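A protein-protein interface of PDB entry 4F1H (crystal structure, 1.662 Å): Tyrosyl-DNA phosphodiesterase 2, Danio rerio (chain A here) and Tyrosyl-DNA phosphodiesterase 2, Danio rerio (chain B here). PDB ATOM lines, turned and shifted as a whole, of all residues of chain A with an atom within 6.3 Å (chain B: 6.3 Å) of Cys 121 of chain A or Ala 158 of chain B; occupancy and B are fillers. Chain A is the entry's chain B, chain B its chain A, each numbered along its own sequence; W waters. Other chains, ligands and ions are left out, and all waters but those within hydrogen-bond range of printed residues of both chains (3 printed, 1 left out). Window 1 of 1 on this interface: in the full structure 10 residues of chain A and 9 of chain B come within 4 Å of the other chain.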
ATOM      1  N   MET A  95       4.249  -3.952 -16.030  1.00  0.00           N
ATOM      2  CA  MET A  95       4.125  -5.357 -16.332  1.00  0.00           C
ATOM      3  C   MET A  95       4.699  -5.670 -17.721  1.00  0.00           C
ATOM      4  O   MET A  95       4.365  -6.704 -18.308  1.00  0.00           O
ATOM      5  CB  MET A  95       2.640  -5.780 -16.298  1.00  0.00           C
ATOM      6  CG  MET A  95       1.924  -5.366 -15.015  1.00  0.00           C
ATOM      7  SD  MET A  95       0.214  -5.911 -14.950  1.00  0.00           S
ATOM      8  CE  MET A  95      -0.355  -4.855 -13.609  1.00  0.00           C
ATOM      9  N   ARG A  97       4.108  -4.514 -20.579  1.00  0.00           N
ATOM     10  CA  ARG A  97       3.145  -4.581 -21.694  1.00  0.00           C
ATOM     11  C   ARG A  97       3.479  -3.598 -22.789  1.00  0.00           C
ATOM     12  O   ARG A  97       4.089  -2.532 -22.563  1.00  0.00           O
ATOM     13  CB  ARG A  97       1.728  -4.323 -21.161  1.00  0.00           C
ATOM     14  CG  ARG A  97       1.375  -5.203 -19.971  1.00  0.00           C
ATOM     15  CD  ARG A  97       1.647  -6.681 -20.237  1.00  0.00           C
ATOM     16  NE  ARG A  97       1.522  -7.498 -19.021  1.00  0.00           N
ATOM     17  CZ  ARG A  97       0.369  -7.826 -18.430  1.00  0.00           C
ATOM     18  NH1 ARG A  97      -0.783  -7.385 -18.925  1.00  0.00           N
ATOM     19  NH2 ARG A  97       0.376  -8.575 -17.322  1.00  0.00           N
ATOM     20  N   LEU A 118      -3.196  -5.998 -22.273  1.00  0.00           N
ATOM     21  CA  LEU A 118      -3.285  -4.752 -21.519  1.00  0.00           C
ATOM     22  C   LEU A 118      -3.129  -5.014 -20.030  1.00  0.00           C
ATOM     23  O   LEU A 118      -3.380  -6.136 -19.522  1.00  0.00           O
ATOM     24  CB  LEU A 118      -4.572  -3.960 -21.773  1.00  0.00           C
ATOM     25  CG  LEU A 118      -4.863  -3.562 -23.229  1.00  0.00           C
ATOM     26  CD1 LEU A 118      -6.083  -2.642 -23.305  1.00  0.00           C
ATOM     27  CD2 LEU A 118      -3.643  -2.971 -23.945  1.00  0.00           C
ATOM     28  N   GLU A 119      -2.705  -3.964 -19.330  1.00  0.00           N
ATOM     29  CA  GLU A 119      -2.395  -4.042 -17.891  1.00  0.00           C
ATOM     30  C   GLU A 119      -3.457  -4.858 -17.143  1.00  0.00           C
ATOM     31  O   GLU A 119      -4.666  -4.646 -17.337  1.00  0.00           O
ATOM     32  CB  GLU A 119      -2.334  -2.629 -17.310  1.00  0.00           C
ATOM     33  CG  GLU A 119      -1.382  -2.536 -16.111  1.00  0.00           C
ATOM     34  CD  GLU A 119       0.073  -2.443 -16.496  1.00  0.00           C
ATOM     35  OE1 GLU A 119       0.439  -2.638 -17.680  1.00  0.00           O
ATOM     36  OE2 GLU A 119       0.859  -2.149 -15.573  1.00  0.00           O
ATOM     37  N   SER A 120      -2.988  -5.791 -16.318  1.00  0.00           N
ATOM     38  CA  SER A 120      -3.820  -6.801 -15.659  1.00  0.00           C
ATOM     39  C   SER A 120      -4.453  -6.322 -14.356  1.00  0.00           C
ATOM     40  O   SER A 120      -3.918  -5.403 -13.707  1.00  0.00           O
ATOM     41  CB  SER A 120      -2.989  -8.061 -15.361  1.00  0.00           C
ATOM     42  OG  SER A 120      -2.525  -8.674 -16.561  1.00  0.00           O
ATOM     43  N   CYS A 121      -5.601  -6.930 -14.036  1.00  0.00           N
ATOM     44  CA  CYS A 121      -6.302  -6.810 -12.732  1.00  0.00           C
ATOM     45  C   CYS A 121      -7.280  -5.640 -12.609  1.00  0.00           C
ATOM     46  O   CYS A 121      -7.102  -4.560 -13.180  1.00  0.00           O
ATOM     47  CB  CYS A 121      -5.327  -6.874 -11.548  1.00  0.00           C
ATOM     48  SG  CYS A 121      -4.455  -8.470 -11.443  1.00  0.00           S
ATOM     49  N   LYS A 122      -8.352  -5.878 -11.863  1.00  0.00           N
ATOM     50  CA  LYS A 122      -9.373  -4.840 -11.691  1.00  0.00           C
ATOM     51  C   LYS A 122      -8.774  -3.523 -11.221  1.00  0.00           C
ATOM     52  O   LYS A 122      -9.116  -2.449 -11.729  1.00  0.00           O
ATOM     53  CB  LYS A 122     -10.426  -5.289 -10.666  1.00  0.00           C
ATOM     54  CG  LYS A 122     -11.587  -4.312 -10.552  1.00  0.00           C
ATOM     55  CD  LYS A 122     -12.499  -4.726  -9.395  1.00  0.00           C
ATOM     56  CE  LYS A 122     -13.571  -3.666  -9.114  1.00  0.00           C
ATOM     57  NZ  LYS A 122     -14.374  -4.036  -7.901  1.00  0.00           N
ATOM     58  N   ASN A 123      -7.841  -3.592 -10.270  1.00  0.00           N
ATOM     59  CA  ASN A 123      -7.292  -2.342  -9.713  1.00  0.00           C
ATOM     60  C   ASN A 123      -6.423  -1.502 -10.649  1.00  0.00           C
ATOM     61  O   ASN A 123      -6.081  -0.373 -10.325  1.00  0.00           O
ATOM     62  CB  ASN A 123      -6.558  -2.579  -8.368  1.00  0.00           C
ATOM     63  CG  ASN A 123      -5.339  -3.513  -8.487  1.00  0.00           C
ATOM     64  OD1 ASN A 123      -4.577  -3.453  -9.442  1.00  0.00           O
ATOM     65  ND2 ASN A 123      -5.150  -4.370  -7.484  1.00  0.00           N
ATOM     66  N   GLN A 124      -6.065  -2.052 -11.808  1.00  0.00           N
ATOM     67  CA  GLN A 124      -5.256  -1.318 -12.781  1.00  0.00           C
ATOM     68  C   GLN A 124      -6.099  -0.714 -13.891  1.00  0.00           C
ATOM     69  O   GLN A 124      -5.604  -0.433 -14.982  1.00  0.00           O
ATOM     70  CB  GLN A 124      -4.188  -2.246 -13.358  1.00  0.00           C
ATOM     71  CG  GLN A 124      -3.097  -2.592 -12.345  1.00  0.00           C
ATOM     72  CD  GLN A 124      -2.467  -1.324 -11.767  1.00  0.00           C
ATOM     73  OE1 GLN A 124      -1.987  -0.468 -12.500  1.00  0.00           O
ATOM     74  NE2 GLN A 124      -2.518  -1.183 -10.432  1.00  0.00           N
ATOM     75  N   SER A 125      -7.377  -0.486 -13.600  1.00  0.00           N
ATOM     76  CA  SER A 125      -8.245   0.227 -14.529  1.00  0.00           C
ATOM     77  C   SER A 125      -7.623   1.485 -15.161  1.00  0.00           C
ATOM     78  O   SER A 125      -7.737   1.712 -16.371  1.00  0.00           O
ATOM     79  CB  SER A 125      -9.568   0.577 -13.812  1.00  0.00           C
ATOM     80  OG  SER A 125     -10.425   1.206 -14.716  1.00  0.00           O
ATOM     81  N   ARG A 128      -4.636   0.513 -17.564  1.00  0.00           N
ATOM     82  CA  ARG A 128      -5.276  -0.217 -18.675  1.00  0.00           C
ATOM     83  C   ARG A 128      -6.034   0.726 -19.617  1.00  0.00           C
ATOM     84  O   ARG A 128      -5.893   0.644 -20.837  1.00  0.00           O
ATOM     85  CB  ARG A 128      -6.203  -1.295 -18.111  1.00  0.00           C
ATOM     86  CG  ARG A 128      -7.062  -1.934 -19.168  1.00  0.00           C
ATOM     87  CD  ARG A 128      -7.690  -3.178 -18.610  1.00  0.00           C
ATOM     88  NE  ARG A 128      -8.532  -2.924 -17.427  1.00  0.00           N
ATOM     89  CZ  ARG A 128      -8.223  -3.315 -16.193  1.00  0.00           C
ATOM     90  NH1 ARG A 128      -7.059  -3.940 -15.941  1.00  0.00           N
ATOM     91  NH2 ARG A 128      -9.096  -3.063 -15.204  1.00  0.00           N
ATOM     92  N   ASN A 155      -8.065  -7.318 -20.961  1.00  0.00           N
ATOM     93  CA  ASN A 155      -8.384  -7.200 -19.538  1.00  0.00           C
ATOM     94  C   ASN A 155      -9.499  -6.210 -19.235  1.00  0.00           C
ATOM     95  O   ASN A 155      -9.679  -5.779 -18.091  1.00  0.00           O
ATOM     96  CB  ASN A 155      -7.111  -6.911 -18.711  1.00  0.00           C
ATOM     97  CG  ASN A 155      -6.372  -8.172 -18.387  1.00  0.00           C
ATOM     98  OD1 ASN A 155      -6.965  -9.123 -17.867  1.00  0.00           O
ATOM     99  ND2 ASN A 155      -5.081  -8.231 -18.732  1.00  0.00           N
ATOM    100  N   ARG A 157     -13.102  -4.513 -18.509  1.00  0.00           N
ATOM    101  CA  ARG A 157     -14.334  -4.919 -17.855  1.00  0.00           C
ATOM    102  C   ARG A 157     -15.401  -3.890 -18.059  1.00  0.00           C
ATOM    103  O   ARG A 157     -15.216  -2.899 -18.778  1.00  0.00           O
ATOM    104  CB  ARG A 157     -14.133  -5.174 -16.365  1.00  0.00           C
ATOM    105  CG  ARG A 157     -13.148  -4.258 -15.718  1.00  0.00           C
ATOM    106  CD  ARG A 157     -11.828  -4.943 -15.649  1.00  0.00           C
ATOM    107  NE  ARG A 157     -11.795  -5.977 -14.623  1.00  0.00           N
ATOM    108  CZ  ARG A 157     -10.768  -6.800 -14.473  1.00  0.00           C
ATOM    109  NH1 ARG A 157     -10.779  -7.721 -13.515  1.00  0.00           N
ATOM    110  NH2 ARG A 157      -9.731  -6.692 -15.303  1.00  0.00           N
ATOM    111  N   GLU A 160     -15.470   0.131 -18.785  1.00  0.00           N
ATOM    112  CA  GLU A 160     -14.197   0.799 -19.071  1.00  0.00           C
ATOM    113  C   GLU A 160     -14.113   1.366 -20.480  1.00  0.00           C
ATOM    114  O   GLU A 160     -13.492   2.403 -20.684  1.00  0.00           O
ATOM    115  CB  GLU A 160     -12.986  -0.103 -18.791  1.00  0.00           C
ATOM    116  CG  GLU A 160     -12.778  -0.312 -17.308  1.00  0.00           C
ATOM    117  CD  GLU A 160     -11.704  -1.338 -16.979  1.00  0.00           C
ATOM    118  OE1 GLU A 160     -11.332  -2.133 -17.868  1.00  0.00           O
ATOM    119  OE2 GLU A 160     -11.252  -1.371 -15.808  1.00  0.00           O
ATOM    120  N   ARG B 156       1.641  -6.456  -5.022  1.00  0.00           N
ATOM    121  CA  ARG B 156       0.483  -5.850  -5.698  1.00  0.00           C
ATOM    122  C   ARG B 156      -0.320  -7.026  -6.275  1.00  0.00           C
ATOM    123  O   ARG B 156       0.280  -8.061  -6.613  1.00  0.00           O
ATOM    124  CB  ARG B 156       1.027  -4.994  -6.833  1.00  0.00           C
ATOM    125  CG  ARG B 156       1.521  -3.636  -6.410  1.00  0.00           C
ATOM    126  CD  ARG B 156       2.812  -3.673  -5.599  1.00  0.00           C
ATOM    127  NE  ARG B 156       3.187  -2.308  -5.253  1.00  0.00           N
ATOM    128  CZ  ARG B 156       4.237  -1.954  -4.523  1.00  0.00           C
ATOM    129  NH1 ARG B 156       5.081  -2.865  -3.971  1.00  0.00           N
ATOM    130  NH2 ARG B 156       4.434  -0.655  -4.343  1.00  0.00           N
ATOM    131  N   ASP B 157      -1.652  -6.903  -6.369  1.00  0.00           N
ATOM    132  CA  ASP B 157      -2.492  -8.015  -6.855  1.00  0.00           C
ATOM    133  C   ASP B 157      -2.004  -8.600  -8.170  1.00  0.00           C
ATOM    134  O   ASP B 157      -2.045  -9.830  -8.365  1.00  0.00           O
ATOM    135  CB  ASP B 157      -3.949  -7.599  -7.084  1.00  0.00           C
ATOM    136  CG  ASP B 157      -4.668  -7.236  -5.817  1.00  0.00           C
ATOM    137  OD1 ASP B 157      -4.140  -7.481  -4.708  1.00  0.00           O
ATOM    138  OD2 ASP B 157      -5.789  -6.702  -5.938  1.00  0.00           O
ATOM    139  N   ALA B 158      -1.599  -7.732  -9.099  1.00  0.00           N
ATOM    140  CA  ALA B 158      -1.152  -8.270 -10.376  1.00  0.00           C
ATOM    141  C   ALA B 158       0.120  -9.109 -10.298  1.00  0.00           C
ATOM    142  O   ALA B 158       0.346 -10.004 -11.120  1.00  0.00           O
ATOM    143  CB  ALA B 158      -0.994  -7.164 -11.366  1.00  0.00           C
ATOM    144  N   GLU B 159       0.965  -8.840  -9.305  1.00  0.00           N
ATOM    145  CA  GLU B 159       2.201  -9.608  -9.195  1.00  0.00           C
ATOM    146  C   GLU B 159       1.916 -11.066  -8.886  1.00  0.00           C
ATOM    147  O   GLU B 159       2.643 -11.960  -9.342  1.00  0.00           O
ATOM    148  CB  GLU B 159       3.124  -8.987  -8.138  1.00  0.00           C
ATOM    149  CG  GLU B 159       3.630  -7.639  -8.582  1.00  0.00           C
ATOM    150  CD  GLU B 159       4.400  -6.836  -7.532  1.00  0.00           C
ATOM    151  OE1 GLU B 159       4.403  -7.194  -6.324  1.00  0.00           O
ATOM    152  OE2 GLU B 159       5.004  -5.804  -7.927  1.00  0.00           O
ATOM    153  N   VAL B 160       0.853 -11.307  -8.111  1.00  0.00           N
ATOM    154  CA  VAL B 160       0.417 -12.656  -7.822  1.00  0.00           C
ATOM    155  C   VAL B 160      -0.199 -13.308  -9.081  1.00  0.00           C
ATOM    156  O   VAL B 160       0.163 -14.433  -9.435  1.00  0.00           O
ATOM    157  CB  VAL B 160      -0.594 -12.664  -6.667  1.00  0.00           C
ATOM    158  CG1 VAL B 160      -1.016 -14.076  -6.363  1.00  0.00           C
ATOM    159  CG2 VAL B 160       0.077 -12.024  -5.439  1.00  0.00           C
ATOM    160  N   ALA B 161      -1.105 -12.605  -9.756  1.00  0.00           N
ATOM    161  CA  ALA B 161      -1.655 -13.153 -11.011  1.00  0.00           C
ATOM    162  C   ALA B 161      -0.517 -13.456 -11.990  1.00  0.00           C
ATOM    163  O   ALA B 161      -0.526 -14.501 -12.656  1.00  0.00           O
ATOM    164  CB  ALA B 161      -2.688 -12.192 -11.639  1.00  0.00           C
ATOM    165  N   ASN B 162       0.474 -12.565 -12.054  1.00  0.00           N
ATOM    166  CA  ASN B 162       1.600 -12.719 -12.987  1.00  0.00           C
ATOM    167  C   ASN B 162       2.655 -13.790 -12.650  1.00  0.00           C
ATOM    168  O   ASN B 162       3.649 -13.920 -13.382  1.00  0.00           O
ATOM    169  CB  ASN B 162       2.244 -11.351 -13.319  1.00  0.00           C
ATOM    170  CG  ASN B 162       1.270 -10.413 -14.044  1.00  0.00           C
ATOM    171  OD1 ASN B 162       0.358 -10.879 -14.727  1.00  0.00           O
ATOM    172  ND2 ASN B 162       1.437  -9.100 -13.868  1.00  0.00           N
ATOM    173  N   VAL B 163       2.438 -14.568 -11.578  1.00  0.00           N
ATOM    174  CA  VAL B 163       3.216 -15.809 -11.365  1.00  0.00           C
ATOM    175  C   VAL B 163       2.307 -17.007 -11.505  1.00  0.00           C
ATOM    176  O   VAL B 163       2.684 -18.139 -11.185  1.00  0.00           O
ATOM    177  CB  VAL B 163       3.925 -15.895 -10.001  1.00  0.00           C
ATOM    178  CG1 VAL B 163       4.779 -14.710  -9.826  1.00  0.00           C
ATOM    179  CG2 VAL B 163       2.913 -16.013  -8.829  1.00  0.00           C
HETATM  180  O   HOH W   1      -2.107  -4.758  -9.162  1.00  0.00           O
HETATM  181  O   HOH W   2      -6.395  -4.164  -5.078  1.00  0.00           O
HETATM  182  O   HOH W   3      -7.608  -6.002  -8.340  1.00  0.00           O
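Printed residues of chain B within 4 Å of Cys 121 of chain A: Ala 158.
Of the printed residues of chain A, Ala 158 of chain B touches Met 95 (3.3 Å) and Cys 121 (3.5 Å).
Of the printed residues of chain A, Asn 162 of chain B touches Met 95 and Arg 97.
Of the printed residues of chain B, Arg 97 of chain A touches Asn 162.
Of the printed residues of chain B, Asn 123 of chain A touches Asp 157 (2.9 Å).
Printed residues of chain B within 4 Å of Met 95 of chain A: Ala 158 (3.3 Å) and Asn 162 (3.6 Å).
Ala 161 of chain B touches none of the printed residues of chain A.
The nearest printed residue of chain B that does not touch Cys 121 of chain A is Asp 157 of chain B (4.1 Å).
Water W2 lies within hydrogen-bond range of ND2 of Asn 123 of chain A and OD2 of Asp 157 of chain B.
Water W1 bridges the side-chain amide oxygen (OD1) of Asn 123 of chain A and the backbone NH (N) of Ala 158 of chain B.
Water W3 lies within hydrogen-bond range of the side-chain amide nitrogen of Asn 123 of chain A (3.1 Å) and the side-chain carboxylate of Asp 157 of chain B (3.1 Å).
The side-chain carboxylate of Asp 157 of chain B sits at hydrogen-bond distance from the side-chain amide nitrogen of Asn 123 of chain A (2.9 Å).
SG of Cys 121 of chain A sits close to N of Ala 158 of chain B (3.8 Å).
SD of Met 95 of chain A is in hydrogen-bond range of ND2 of Asn 162 of chain B (3.6 Å).
OD1 of Asn 162 of chain B sits at hydrogen-bond distance from NH2 of Arg 97 of chain A (3.5 Å).
Among the printed residues, pairs that only touch across the chains: Met 95 of chain A with Ala 158 of chain B (3.3 Å).
O of Ala 158 of chain B sits at hydrogen-bond distance from ND2 of Asn 162 of chain B, 3.1 Å away.
O of Met 95 of chain A is in hydrogen-bond range of NE of Arg 97 of chain A, at 3.0 Å.
SD of Met 95 of chain A is in hydrogen-bond range of N of Ser 120 of chain A, 3.5 Å away.
The guanidinium group (NH2) of Arg 97 of chain A lies within hydrogen-bond range of the side-chain hydroxyl (OG) of Ser 120 of chain A.
The backbone carbonyl oxygen (O) of Cys 121 of chain A is in hydrogen-bond range of the guanidinium group (NH1) of Arg 128 of chain A, at 2.8 Å.
The side-chain amide oxygen (OD1) of Asn 123 of chain A is in hydrogen-bond range of the side-chain amide nitrogen (NE2) of Gln 124 of chain A, at 3.2 Å.
Along chain B the printed residues that touch a printed residue of chain A span positions 157 to 162.
Among the printed residues, 5 pairs touch across the chains.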
